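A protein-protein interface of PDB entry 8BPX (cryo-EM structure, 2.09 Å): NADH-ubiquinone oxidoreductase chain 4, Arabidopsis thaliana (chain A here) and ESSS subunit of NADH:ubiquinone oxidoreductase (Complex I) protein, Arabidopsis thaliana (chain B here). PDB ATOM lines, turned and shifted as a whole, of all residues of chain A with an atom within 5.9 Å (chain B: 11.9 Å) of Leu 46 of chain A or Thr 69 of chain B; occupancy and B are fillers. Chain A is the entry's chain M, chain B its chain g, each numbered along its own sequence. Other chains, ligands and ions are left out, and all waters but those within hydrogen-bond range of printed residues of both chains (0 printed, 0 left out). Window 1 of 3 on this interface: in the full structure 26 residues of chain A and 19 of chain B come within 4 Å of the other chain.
CD1 of Leu 46 of chain A touches O of Pro 65 of chain B, at 3.8 Å.
OG1 of Thr 69 of chain B touches CD1 of Leu 46 of chain A (3.4 Å).
Phe 49 of chain A touches Thr 73 of chain B (CE2 to OG1, 3.3 Å).
Leu 50 of chain A touches Leu 72 of chain B.
Leu 50 of chain A touches Thr 73 of chain B.
O of Pro 65 of chain B lies within hydrogen-bond range of OG1 of Thr 69 of chain B (3.1 Å).
The backbone carbonyl oxygen (O) of Thr 69 of chain B is in hydrogen-bond range of the side-chain hydroxyl (OG1) of Thr 73 of chain B (2.8 Å).
No residue of chain B comes within 4 Å of Cys 43 of chain A.
No residue of chain B comes within 4 Å of Ala 44 of chain A.
No residue of chain B comes within 4 Å of Ser 45 of chain A.
Leu 46 of chain A touches just these residues of chain B: Pro 65 and Thr 69.
No residue of chain B comes within 4 Å of Ile 47 of chain A.
Leu 50 of chain A touches two residues of chain B.
No residue of chain B comes within 4 Å of Pro 102 of chain A.
Glu 60 of chain B touches none of the printed residues of chain A.
Trp 62 of chain B touches none of the printed residues of chain A.
Printed residues of chain A within 4 Å of Pro 65 of chain B: Leu 46.
Of chain A, only Leu 46 (3.4 Å) comes within 4 Å of Thr 69 of chain B.
Of the printed residues of chain A, Leu 72 of chain B touches Leu 50.
Of the printed residues of chain A, Thr 73 of chain B touches Phe 49 and Leu 50.
The nearest residue of chain A that does not touch Thr 69 of chain B is Leu 50 of chain A (4.1 Å).
Hydrophobic or aromatic side chains of chain A within 4 Å of the printed part of chain B: Leu 46, Phe 49 and Leu 50.
Among the printed residues, 5 pairs touch across the chains.
Among the printed residues, no Asp or Glu carboxylate lies within 4 Å of a Lys or Arg side-chain nitrogen of the other chain.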
ATOM      1  N   GLY A  41       5.152 -16.692  23.367  1.00  0.00           N
ATOM      2  CA  GLY A  41       5.346 -16.214  24.729  1.00  0.00           C
ATOM      3  C   GLY A  41       6.658 -16.687  25.329  1.00  0.00           C
ATOM      4  O   GLY A  41       7.420 -15.897  25.906  1.00  0.00           O
ATOM      5  N   LEU A  42       6.947 -17.985  25.182  1.00  0.00           N
ATOM      6  CA  LEU A  42       8.189 -18.534  25.715  1.00  0.00           C
ATOM      7  C   LEU A  42       9.401 -17.823  25.126  1.00  0.00           C
ATOM      8  O   LEU A  42      10.340 -17.467  25.849  1.00  0.00           O
ATOM      9  CB  LEU A  42       8.260 -20.034  25.428  1.00  0.00           C
ATOM     10  CG  LEU A  42       9.542 -20.744  25.868  1.00  0.00           C
ATOM     11  CD1 LEU A  42       9.714 -20.670  27.376  1.00  0.00           C
ATOM     12  CD2 LEU A  42       9.568 -22.185  25.380  1.00  0.00           C
ATOM     13  N   CYS A  43       9.391 -17.595  23.811  1.00  0.00           N
ATOM     14  CA  CYS A  43      10.553 -17.008  23.155  1.00  0.00           C
ATOM     15  C   CYS A  43      10.740 -15.552  23.550  1.00  0.00           C
ATOM     16  O   CYS A  43      11.875 -15.103  23.749  1.00  0.00           O
ATOM     17  CB  CYS A  43      10.421 -17.150  21.641  1.00  0.00           C
ATOM     18  SG  CYS A  43      10.876 -18.787  21.051  1.00  0.00           S
ATOM     19  N   ALA A  44       9.646 -14.797  23.675  1.00  0.00           N
ATOM     20  CA  ALA A  44       9.766 -13.420  24.143  1.00  0.00           C
ATOM     21  C   ALA A  44      10.392 -13.375  25.533  1.00  0.00           C
ATOM     22  O   ALA A  44      11.312 -12.583  25.793  1.00  0.00           O
ATOM     23  CB  ALA A  44       8.393 -12.748  24.146  1.00  0.00           C
ATOM     24  N   SER A  45       9.923 -14.243  26.435  1.00  0.00           N
ATOM     25  CA  SER A  45      10.473 -14.249  27.789  1.00  0.00           C
ATOM     26  C   SER A  45      11.951 -14.636  27.790  1.00  0.00           C
ATOM     27  O   SER A  45      12.764 -14.031  28.505  1.00  0.00           O
ATOM     28  CB  SER A  45       9.655 -15.182  28.679  1.00  0.00           C
ATOM     29  OG  SER A  45       9.570 -16.481  28.124  1.00  0.00           O
ATOM     30  N   LEU A  46      12.324 -15.634  26.981  1.00  0.00           N
ATOM     31  CA  LEU A  46      13.720 -16.071  26.939  1.00  0.00           C
ATOM     32  C   LEU A  46      14.629 -14.983  26.373  1.00  0.00           C
ATOM     33  O   LEU A  46      15.750 -14.782  26.863  1.00  0.00           O
ATOM     34  CB  LEU A  46      13.841 -17.350  26.114  1.00  0.00           C
ATOM     35  CG  LEU A  46      13.255 -18.632  26.709  1.00  0.00           C
ATOM     36  CD1 LEU A  46      13.195 -19.713  25.645  1.00  0.00           C
ATOM     37  CD2 LEU A  46      14.042 -19.106  27.919  1.00  0.00           C
ATOM     38  N   ILE A  47      14.171 -14.277  25.335  1.00  0.00           N
ATOM     39  CA  ILE A  47      14.964 -13.190  24.768  1.00  0.00           C
ATOM     40  C   ILE A  47      15.153 -12.080  25.793  1.00  0.00           C
ATOM     41  O   ILE A  47      16.236 -11.490  25.897  1.00  0.00           O
ATOM     42  CB  ILE A  47      14.317 -12.664  23.474  1.00  0.00           C
ATOM     43  CG1 ILE A  47      14.367 -13.727  22.377  1.00  0.00           C
ATOM     44  CG2 ILE A  47      15.021 -11.412  22.994  1.00  0.00           C
ATOM     45  CD1 ILE A  47      13.289 -13.574  21.348  1.00  0.00           C
ATOM     46  N   THR A  48      14.105 -11.776  26.565  1.00  0.00           N
ATOM     47  CA  THR A  48      14.249 -10.783  27.627  1.00  0.00           C
ATOM     48  C   THR A  48      15.285 -11.223  28.658  1.00  0.00           C
ATOM     49  O   THR A  48      16.093 -10.411  29.131  1.00  0.00           O
ATOM     50  CB  THR A  48      12.895 -10.528  28.291  1.00  0.00           C
ATOM     51  OG1 THR A  48      11.875 -10.467  27.286  1.00  0.00           O
ATOM     52  CG2 THR A  48      12.911  -9.222  29.063  1.00  0.00           C
ATOM     53  N   PHE A  49      15.283 -12.511  29.011  1.00  0.00           N
ATOM     54  CA  PHE A  49      16.271 -13.021  29.962  1.00  0.00           C
ATOM     55  C   PHE A  49      17.695 -12.857  29.429  1.00  0.00           C
ATOM     56  O   PHE A  49      18.601 -12.425  30.157  1.00  0.00           O
ATOM     57  CB  PHE A  49      15.975 -14.487  30.277  1.00  0.00           C
ATOM     58  CG  PHE A  49      17.019 -15.150  31.125  1.00  0.00           C
ATOM     59  CD1 PHE A  49      17.319 -14.664  32.386  1.00  0.00           C
ATOM     60  CD2 PHE A  49      17.706 -16.259  30.657  1.00  0.00           C
ATOM     61  CE1 PHE A  49      18.278 -15.275  33.167  1.00  0.00           C
ATOM     62  CE2 PHE A  49      18.667 -16.873  31.433  1.00  0.00           C
ATOM     63  CZ  PHE A  49      18.957 -16.382  32.688  1.00  0.00           C
ATOM     64  N   LEU A  50      17.911 -13.197  28.156  1.00  0.00           N
ATOM     65  CA  LEU A  50      19.248 -13.050  27.580  1.00  0.00           C
ATOM     66  C   LEU A  50      19.668 -11.583  27.529  1.00  0.00           C
ATOM     67  O   LEU A  50      20.838 -11.250  27.766  1.00  0.00           O
ATOM     68  CB  LEU A  50      19.300 -13.674  26.187  1.00  0.00           C
ATOM     69  CG  LEU A  50      19.079 -15.186  26.117  1.00  0.00           C
ATOM     70  CD1 LEU A  50      18.934 -15.634  24.672  1.00  0.00           C
ATOM     71  CD2 LEU A  50      20.200 -15.946  26.814  1.00  0.00           C
ATOM     72  N   TYR A  51      18.721 -10.696  27.218  1.00  0.00           N
ATOM     73  CA  TYR A  51      18.995  -9.263  27.217  1.00  0.00           C
ATOM     74  C   TYR A  51      19.456  -8.790  28.594  1.00  0.00           C
ATOM     75  O   TYR A  51      20.415  -8.013  28.709  1.00  0.00           O
ATOM     76  CB  TYR A  51      17.733  -8.526  26.770  1.00  0.00           C
ATOM     77  CG  TYR A  51      17.926  -7.116  26.274  1.00  0.00           C
ATOM     78  CD1 TYR A  51      18.403  -6.123  27.114  1.00  0.00           C
ATOM     79  CD2 TYR A  51      17.591  -6.770  24.974  1.00  0.00           C
ATOM     80  CE1 TYR A  51      18.564  -4.838  26.670  1.00  0.00           C
ATOM     81  CE2 TYR A  51      17.748  -5.482  24.520  1.00  0.00           C
ATOM     82  CZ  TYR A  51      18.234  -4.517  25.374  1.00  0.00           C
ATOM     83  OH  TYR A  51      18.397  -3.227  24.934  1.00  0.00           O
ATOM     84  N   PRO A 102       9.968 -16.715  32.333  1.00  0.00           N
ATOM     85  CA  PRO A 102       9.902 -17.937  31.511  1.00  0.00           C
ATOM     86  C   PRO A 102       9.599 -19.182  32.318  1.00  0.00           C
ATOM     87  O   PRO A 102       8.942 -20.096  31.808  1.00  0.00           O
ATOM     88  CB  PRO A 102      11.299 -18.018  30.875  1.00  0.00           C
ATOM     89  CG  PRO A 102      11.853 -16.665  30.966  1.00  0.00           C
ATOM     90  CD  PRO A 102      11.252 -16.017  32.164  1.00  0.00           C
ATOM     91  N   TRP B  59      10.755 -34.452  20.160  1.00  0.00           N
ATOM     92  CA  TRP B  59      11.018 -33.362  21.095  1.00  0.00           C
ATOM     93  C   TRP B  59       9.780 -32.495  21.267  1.00  0.00           C
ATOM     94  O   TRP B  59       9.152 -32.095  20.284  1.00  0.00           O
ATOM     95  CB  TRP B  59      12.181 -32.497  20.608  1.00  0.00           C
ATOM     96  CG  TRP B  59      13.534 -33.038  20.923  1.00  0.00           C
ATOM     97  CD1 TRP B  59      13.856 -34.332  21.207  1.00  0.00           C
ATOM     98  CD2 TRP B  59      14.759 -32.299  20.976  1.00  0.00           C
ATOM     99  NE1 TRP B  59      15.204 -34.443  21.441  1.00  0.00           N
ATOM    100  CE2 TRP B  59      15.782 -33.209  21.302  1.00  0.00           C
ATOM    101  CE3 TRP B  59      15.088 -30.955  20.781  1.00  0.00           C
ATOM    102  CZ2 TRP B  59      17.112 -32.821  21.438  1.00  0.00           C
ATOM    103  CZ3 TRP B  59      16.410 -30.570  20.915  1.00  0.00           C
ATOM    104  CH2 TRP B  59      17.404 -31.498  21.244  1.00  0.00           C
ATOM    105  N   GLU B  60       9.446 -32.182  22.513  1.00  0.00           N
ATOM    106  CA  GLU B  60       8.359 -31.243  22.747  1.00  0.00           C
ATOM    107  C   GLU B  60       8.767 -29.838  22.311  1.00  0.00           C
ATOM    108  O   GLU B  60       9.949 -29.515  22.180  1.00  0.00           O
ATOM    109  CB  GLU B  60       7.933 -31.258  24.211  1.00  0.00           C
ATOM    110  CG  GLU B  60       7.564 -32.633  24.730  1.00  0.00           C
ATOM    111  CD  GLU B  60       6.562 -32.583  25.868  1.00  0.00           C
ATOM    112  OE1 GLU B  60       6.836 -31.897  26.873  1.00  0.00           O
ATOM    113  OE2 GLU B  60       5.503 -33.237  25.762  1.00  0.00           O
ATOM    114  N   ASP B  61       7.754 -28.999  22.084  1.00  0.00           N
ATOM    115  CA  ASP B  61       7.971 -27.689  21.476  1.00  0.00           C
ATOM    116  C   ASP B  61       8.893 -26.808  22.315  1.00  0.00           C
ATOM    117  O   ASP B  61       9.630 -25.984  21.766  1.00  0.00           O
ATOM    118  CB  ASP B  61       6.630 -26.984  21.266  1.00  0.00           C
ATOM    119  CG  ASP B  61       5.951 -27.382  19.966  1.00  0.00           C
ATOM    120  OD1 ASP B  61       4.927 -26.758  19.622  1.00  0.00           O
ATOM    121  OD2 ASP B  61       6.427 -28.320  19.299  1.00  0.00           O
ATOM    122  N   TRP B  62       8.860 -26.956  23.638  1.00  0.00           N
ATOM    123  CA  TRP B  62       9.662 -26.105  24.506  1.00  0.00           C
ATOM    124  C   TRP B  62      11.137 -26.492  24.532  1.00  0.00           C
ATOM    125  O   TRP B  62      11.961 -25.682  24.960  1.00  0.00           O
ATOM    126  CB  TRP B  62       9.099 -26.135  25.932  1.00  0.00           C
ATOM    127  CG  TRP B  62       9.089 -27.509  26.521  1.00  0.00           C
ATOM    128  CD1 TRP B  62       8.066 -28.407  26.479  1.00  0.00           C
ATOM    129  CD2 TRP B  62      10.158 -28.156  27.222  1.00  0.00           C
ATOM    130  NE1 TRP B  62       8.426 -29.567  27.110  1.00  0.00           N
ATOM    131  CE2 TRP B  62       9.706 -29.440  27.578  1.00  0.00           C
ATOM    132  CE3 TRP B  62      11.450 -27.769  27.590  1.00  0.00           C
ATOM    133  CZ2 TRP B  62      10.501 -30.344  28.274  1.00  0.00           C
ATOM    134  CZ3 TRP B  62      12.236 -28.667  28.285  1.00  0.00           C
ATOM    135  CH2 TRP B  62      11.759 -29.940  28.621  1.00  0.00           C
ATOM    136  N   GLU B  63      11.484 -27.696  24.068  1.00  0.00           N
ATOM    137  CA  GLU B  63      12.812 -28.255  24.322  1.00  0.00           C
ATOM    138  C   GLU B  63      13.909 -27.449  23.634  1.00  0.00           C
ATOM    139  O   GLU B  63      14.851 -26.988  24.282  1.00  0.00           O
ATOM    140  CB  GLU B  63      12.854 -29.715  23.874  1.00  0.00           C
ATOM    141  CG  GLU B  63      11.863 -30.607  24.604  1.00  0.00           C
ATOM    142  CD  GLU B  63      12.403 -31.993  24.886  1.00  0.00           C
ATOM    143  OE1 GLU B  63      13.582 -32.120  25.268  1.00  0.00           O
ATOM    144  OE2 GLU B  63      11.643 -32.960  24.703  1.00  0.00           O
ATOM    145  N   LEU B  64      13.812 -27.284  22.317  1.00  0.00           N
ATOM    146  CA  LEU B  64      14.861 -26.579  21.581  1.00  0.00           C
ATOM    147  C   LEU B  64      15.047 -25.137  22.038  1.00  0.00           C
ATOM    148  O   LEU B  64      16.201 -24.735  22.270  1.00  0.00           O
ATOM    149  CB  LEU B  64      14.578 -26.658  20.076  1.00  0.00           C
ATOM    150  CG  LEU B  64      15.699 -26.191  19.144  1.00  0.00           C
ATOM    151  CD1 LEU B  64      17.016 -26.879  19.482  1.00  0.00           C
ATOM    152  CD2 LEU B  64      15.332 -26.418  17.688  1.00  0.00           C
ATOM    153  N   PRO B  65      13.998 -24.306  22.173  1.00  0.00           N
ATOM    154  CA  PRO B  65      14.229 -22.939  22.669  1.00  0.00           C
ATOM    155  C   PRO B  65      14.888 -22.904  24.035  1.00  0.00           C
ATOM    156  O   PRO B  65      15.805 -22.106  24.256  1.00  0.00           O
ATOM    157  CB  PRO B  65      12.817 -22.335  22.706  1.00  0.00           C
ATOM    158  CG  PRO B  65      12.019 -23.161  21.777  1.00  0.00           C
ATOM    159  CD  PRO B  65      12.572 -24.539  21.881  1.00  0.00           C
ATOM    160  N   CYS B  66      14.474 -23.786  24.944  1.00  0.00           N
ATOM    161  CA  CYS B  66      15.041 -23.788  26.287  1.00  0.00           C
ATOM    162  C   CYS B  66      16.493 -24.246  26.277  1.00  0.00           C
ATOM    163  O   CYS B  66      17.328 -23.672  26.980  1.00  0.00           O
ATOM    164  CB  CYS B  66      14.199 -24.663  27.213  1.00  0.00           C
ATOM    165  SG  CYS B  66      12.700 -23.857  27.823  1.00  0.00           S
ATOM    166  N   TYR B  67      16.816 -25.266  25.479  1.00  0.00           N
ATOM    167  CA  TYR B  67      18.193 -25.751  25.421  1.00  0.00           C
ATOM    168  C   TYR B  67      19.116 -24.718  24.786  1.00  0.00           C
ATOM    169  O   TYR B  67      20.252 -24.532  25.237  1.00  0.00           O
ATOM    170  CB  TYR B  67      18.267 -27.074  24.657  1.00  0.00           C
ATOM    171  CG  TYR B  67      17.481 -28.205  25.277  1.00  0.00           C
ATOM    172  CD1 TYR B  67      17.166 -28.205  26.631  1.00  0.00           C
ATOM    173  CD2 TYR B  67      17.040 -29.265  24.502  1.00  0.00           C
ATOM    174  CE1 TYR B  67      16.441 -29.234  27.191  1.00  0.00           C
ATOM    175  CE2 TYR B  67      16.320 -30.294  25.049  1.00  0.00           C
ATOM    176  CZ  TYR B  67      16.020 -30.280  26.391  1.00  0.00           C
ATOM    177  OH  TYR B  67      15.297 -31.315  26.930  1.00  0.00           O
ATOM    178  N   ILE B  68      18.650 -24.038  23.736  1.00  0.00           N
ATOM    179  CA  ILE B  68      19.455 -22.991  23.118  1.00  0.00           C
ATOM    180  C   ILE B  68      19.638 -21.820  24.075  1.00  0.00           C
ATOM    181  O   ILE B  68      20.728 -21.243  24.165  1.00  0.00           O
ATOM    182  CB  ILE B  68      18.836 -22.553  21.777  1.00  0.00           C
ATOM    183  CG1 ILE B  68      18.965 -23.679  20.750  1.00  0.00           C
ATOM    184  CG2 ILE B  68      19.469 -21.256  21.273  1.00  0.00           C
ATOM    185  CD1 ILE B  68      18.234 -23.412  19.471  1.00  0.00           C
ATOM    186  N   THR B  69      18.591 -21.473  24.828  1.00  0.00           N
ATOM    187  CA  THR B  69      18.728 -20.442  25.847  1.00  0.00           C
ATOM    188  C   THR B  69      19.740 -20.853  26.910  1.00  0.00           C
ATOM    189  O   THR B  69      20.548 -20.035  27.351  1.00  0.00           O
ATOM    190  CB  THR B  69      17.371 -20.147  26.487  1.00  0.00           C
ATOM    191  OG1 THR B  69      16.557 -19.410  25.569  1.00  0.00           O
ATOM    192  CG2 THR B  69      17.549 -19.316  27.747  1.00  0.00           C
ATOM    193  N   SER B  70      19.714 -22.121  27.328  1.00  0.00           N
ATOM    194  CA  SER B  70      20.643 -22.594  28.352  1.00  0.00           C
ATOM    195  C   SER B  70      22.081 -22.549  27.857  1.00  0.00           C
ATOM    196  O   SER B  70      22.987 -22.123  28.587  1.00  0.00           O
ATOM    197  CB  SER B  70      20.274 -24.014  28.776  1.00  0.00           C
ATOM    198  OG  SER B  70      19.097 -24.022  29.553  1.00  0.00           O
ATOM    199  N   PHE B  71      22.305 -22.982  26.617  1.00  0.00           N
ATOM    200  CA  PHE B  71      23.636 -22.915  26.028  1.00  0.00           C
ATOM    201  C   PHE B  71      24.121 -21.476  25.917  1.00  0.00           C
ATOM    202  O   PHE B  71      25.273 -21.174  26.249  1.00  0.00           O
ATOM    203  CB  PHE B  71      23.621 -23.582  24.656  1.00  0.00           C
ATOM    204  CG  PHE B  71      24.868 -23.362  23.865  1.00  0.00           C
ATOM    205  CD1 PHE B  71      26.017 -24.082  24.145  1.00  0.00           C
ATOM    206  CD2 PHE B  71      24.902 -22.422  22.850  1.00  0.00           C
ATOM    207  CE1 PHE B  71      27.172 -23.879  23.420  1.00  0.00           C
ATOM    208  CE2 PHE B  71      26.054 -22.216  22.122  1.00  0.00           C
ATOM    209  CZ  PHE B  71      27.189 -22.948  22.409  1.00  0.00           C
ATOM    210  N   LEU B  72      23.253 -20.573  25.452  1.00  0.00           N
ATOM    211  CA  LEU B  72      23.631 -19.170  25.332  1.00  0.00           C
ATOM    212  C   LEU B  72      23.892 -18.551  26.698  1.00  0.00           C
ATOM    213  O   LEU B  72      24.775 -17.707  26.840  1.00  0.00           O
ATOM    214  CB  LEU B  72      22.546 -18.395  24.587  1.00  0.00           C
ATOM    215  CG  LEU B  72      22.449 -18.599  23.075  1.00  0.00           C
ATOM    216  CD1 LEU B  72      21.551 -17.550  22.459  1.00  0.00           C
ATOM    217  CD2 LEU B  72      23.832 -18.577  22.431  1.00  0.00           C
ATOM    218  N   THR B  73      23.126 -18.957  27.710  1.00  0.00           N
ATOM    219  CA  THR B  73      23.344 -18.478  29.070  1.00  0.00           C
ATOM    220  C   THR B  73      24.714 -18.902  29.572  1.00  0.00           C
ATOM    221  O   THR B  73      25.478 -18.089  30.106  1.00  0.00           O
ATOM    222  CB  THR B  73      22.248 -19.021  29.992  1.00  0.00           C
ATOM    223  OG1 THR B  73      20.982 -18.461  29.627  1.00  0.00           O
ATOM    224  CG2 THR B  73      22.544 -18.695  31.446  1.00  0.00           C
ATOM    225  N   ILE B  74      25.047 -20.181  29.386  1.00  0.00           N
ATOM    226  CA  ILE B  74      26.350 -20.689  29.801  1.00  0.00           C
ATOM    227  C   ILE B  74      27.461 -19.936  29.079  1.00  0.00           C
ATOM    228  O   ILE B  74      28.425 -19.479  29.698  1.00  0.00           O
ATOM    229  CB  ILE B  74      26.436 -22.209  29.558  1.00  0.00           C
ATOM    230  CG1 ILE B  74      26.017 -22.996  30.803  1.00  0.00           C
ATOM    231  CG2 ILE B  74      27.831 -22.622  29.120  1.00  0.00           C
ATOM    232  CD1 ILE B  74      24.768 -22.510  31.483  1.00  0.00           C
ATOM    233  N   VAL B  75      27.322 -19.763  27.765  1.00  0.00           N
ATOM    234  CA  VAL B  75      28.376 -19.116  26.988  1.00  0.00           C
ATOM    235  C   VAL B  75      28.525 -17.655  27.399  1.00  0.00           C
ATOM    236  O   VAL B  75      29.633 -17.186  27.676  1.00  0.00           O
ATOM    237  CB  VAL B  75      28.091 -19.258  25.482  1.00  0.00           C
ATOM    238  CG1 VAL B  75      28.824 -18.183  24.699  1.00  0.00           C
ATOM    239  CG2 VAL B  75      28.478 -20.647  24.999  1.00  0.00           C
ATOM    240  N   ILE B  76      27.407 -16.929  27.479  1.00  0.00           N
ATOM    241  CA  ILE B  76      27.443 -15.511  27.814  1.00  0.00           C
ATOM    242  C   ILE B  76      28.053 -15.308  29.194  1.00  0.00           C
ATOM    243  O   ILE B  76      28.978 -14.511  29.362  1.00  0.00           O
ATOM    244  CB  ILE B  76      26.030 -14.905  27.715  1.00  0.00           C
ATOM    245  CG1 ILE B  76      25.699 -14.571  26.260  1.00  0.00           C
ATOM    246  CG2 ILE B  76      25.898 -13.656  28.572  1.00  0.00           C
ATOM    247  CD1 ILE B  76      24.233 -14.336  26.014  1.00  0.00           C
ATOM    248  N   LEU B  77      27.582 -16.049  30.198  1.00  0.00           N
ATOM    249  CA  LEU B  77      28.111 -15.828  31.540  1.00  0.00           C
ATOM    250  C   LEU B  77      29.563 -16.284  31.648  1.00  0.00           C
ATOM    251  O   LEU B  77      30.429 -15.515  32.083  1.00  0.00           O
ATOM    252  CB  LEU B  77      27.227 -16.521  32.578  1.00  0.00           C
ATOM    253  CG  LEU B  77      25.904 -15.779  32.806  1.00  0.00           C
ATOM    254  CD1 LEU B  77      25.069 -16.416  33.910  1.00  0.00           C
ATOM    255  CD2 LEU B  77      26.139 -14.302  33.079  1.00  0.00           C
ATOM    256  N   GLY B  78      29.863 -17.510  31.206  1.00  0.00           N
ATOM    257  CA  GLY B  78      31.199 -18.060  31.325  1.00  0.00           C
ATOM    258  C   GLY B  78      32.260 -17.323  30.536  1.00  0.00           C
ATOM    259  O   GLY B  78      33.426 -17.335  30.939  1.00  0.00           O
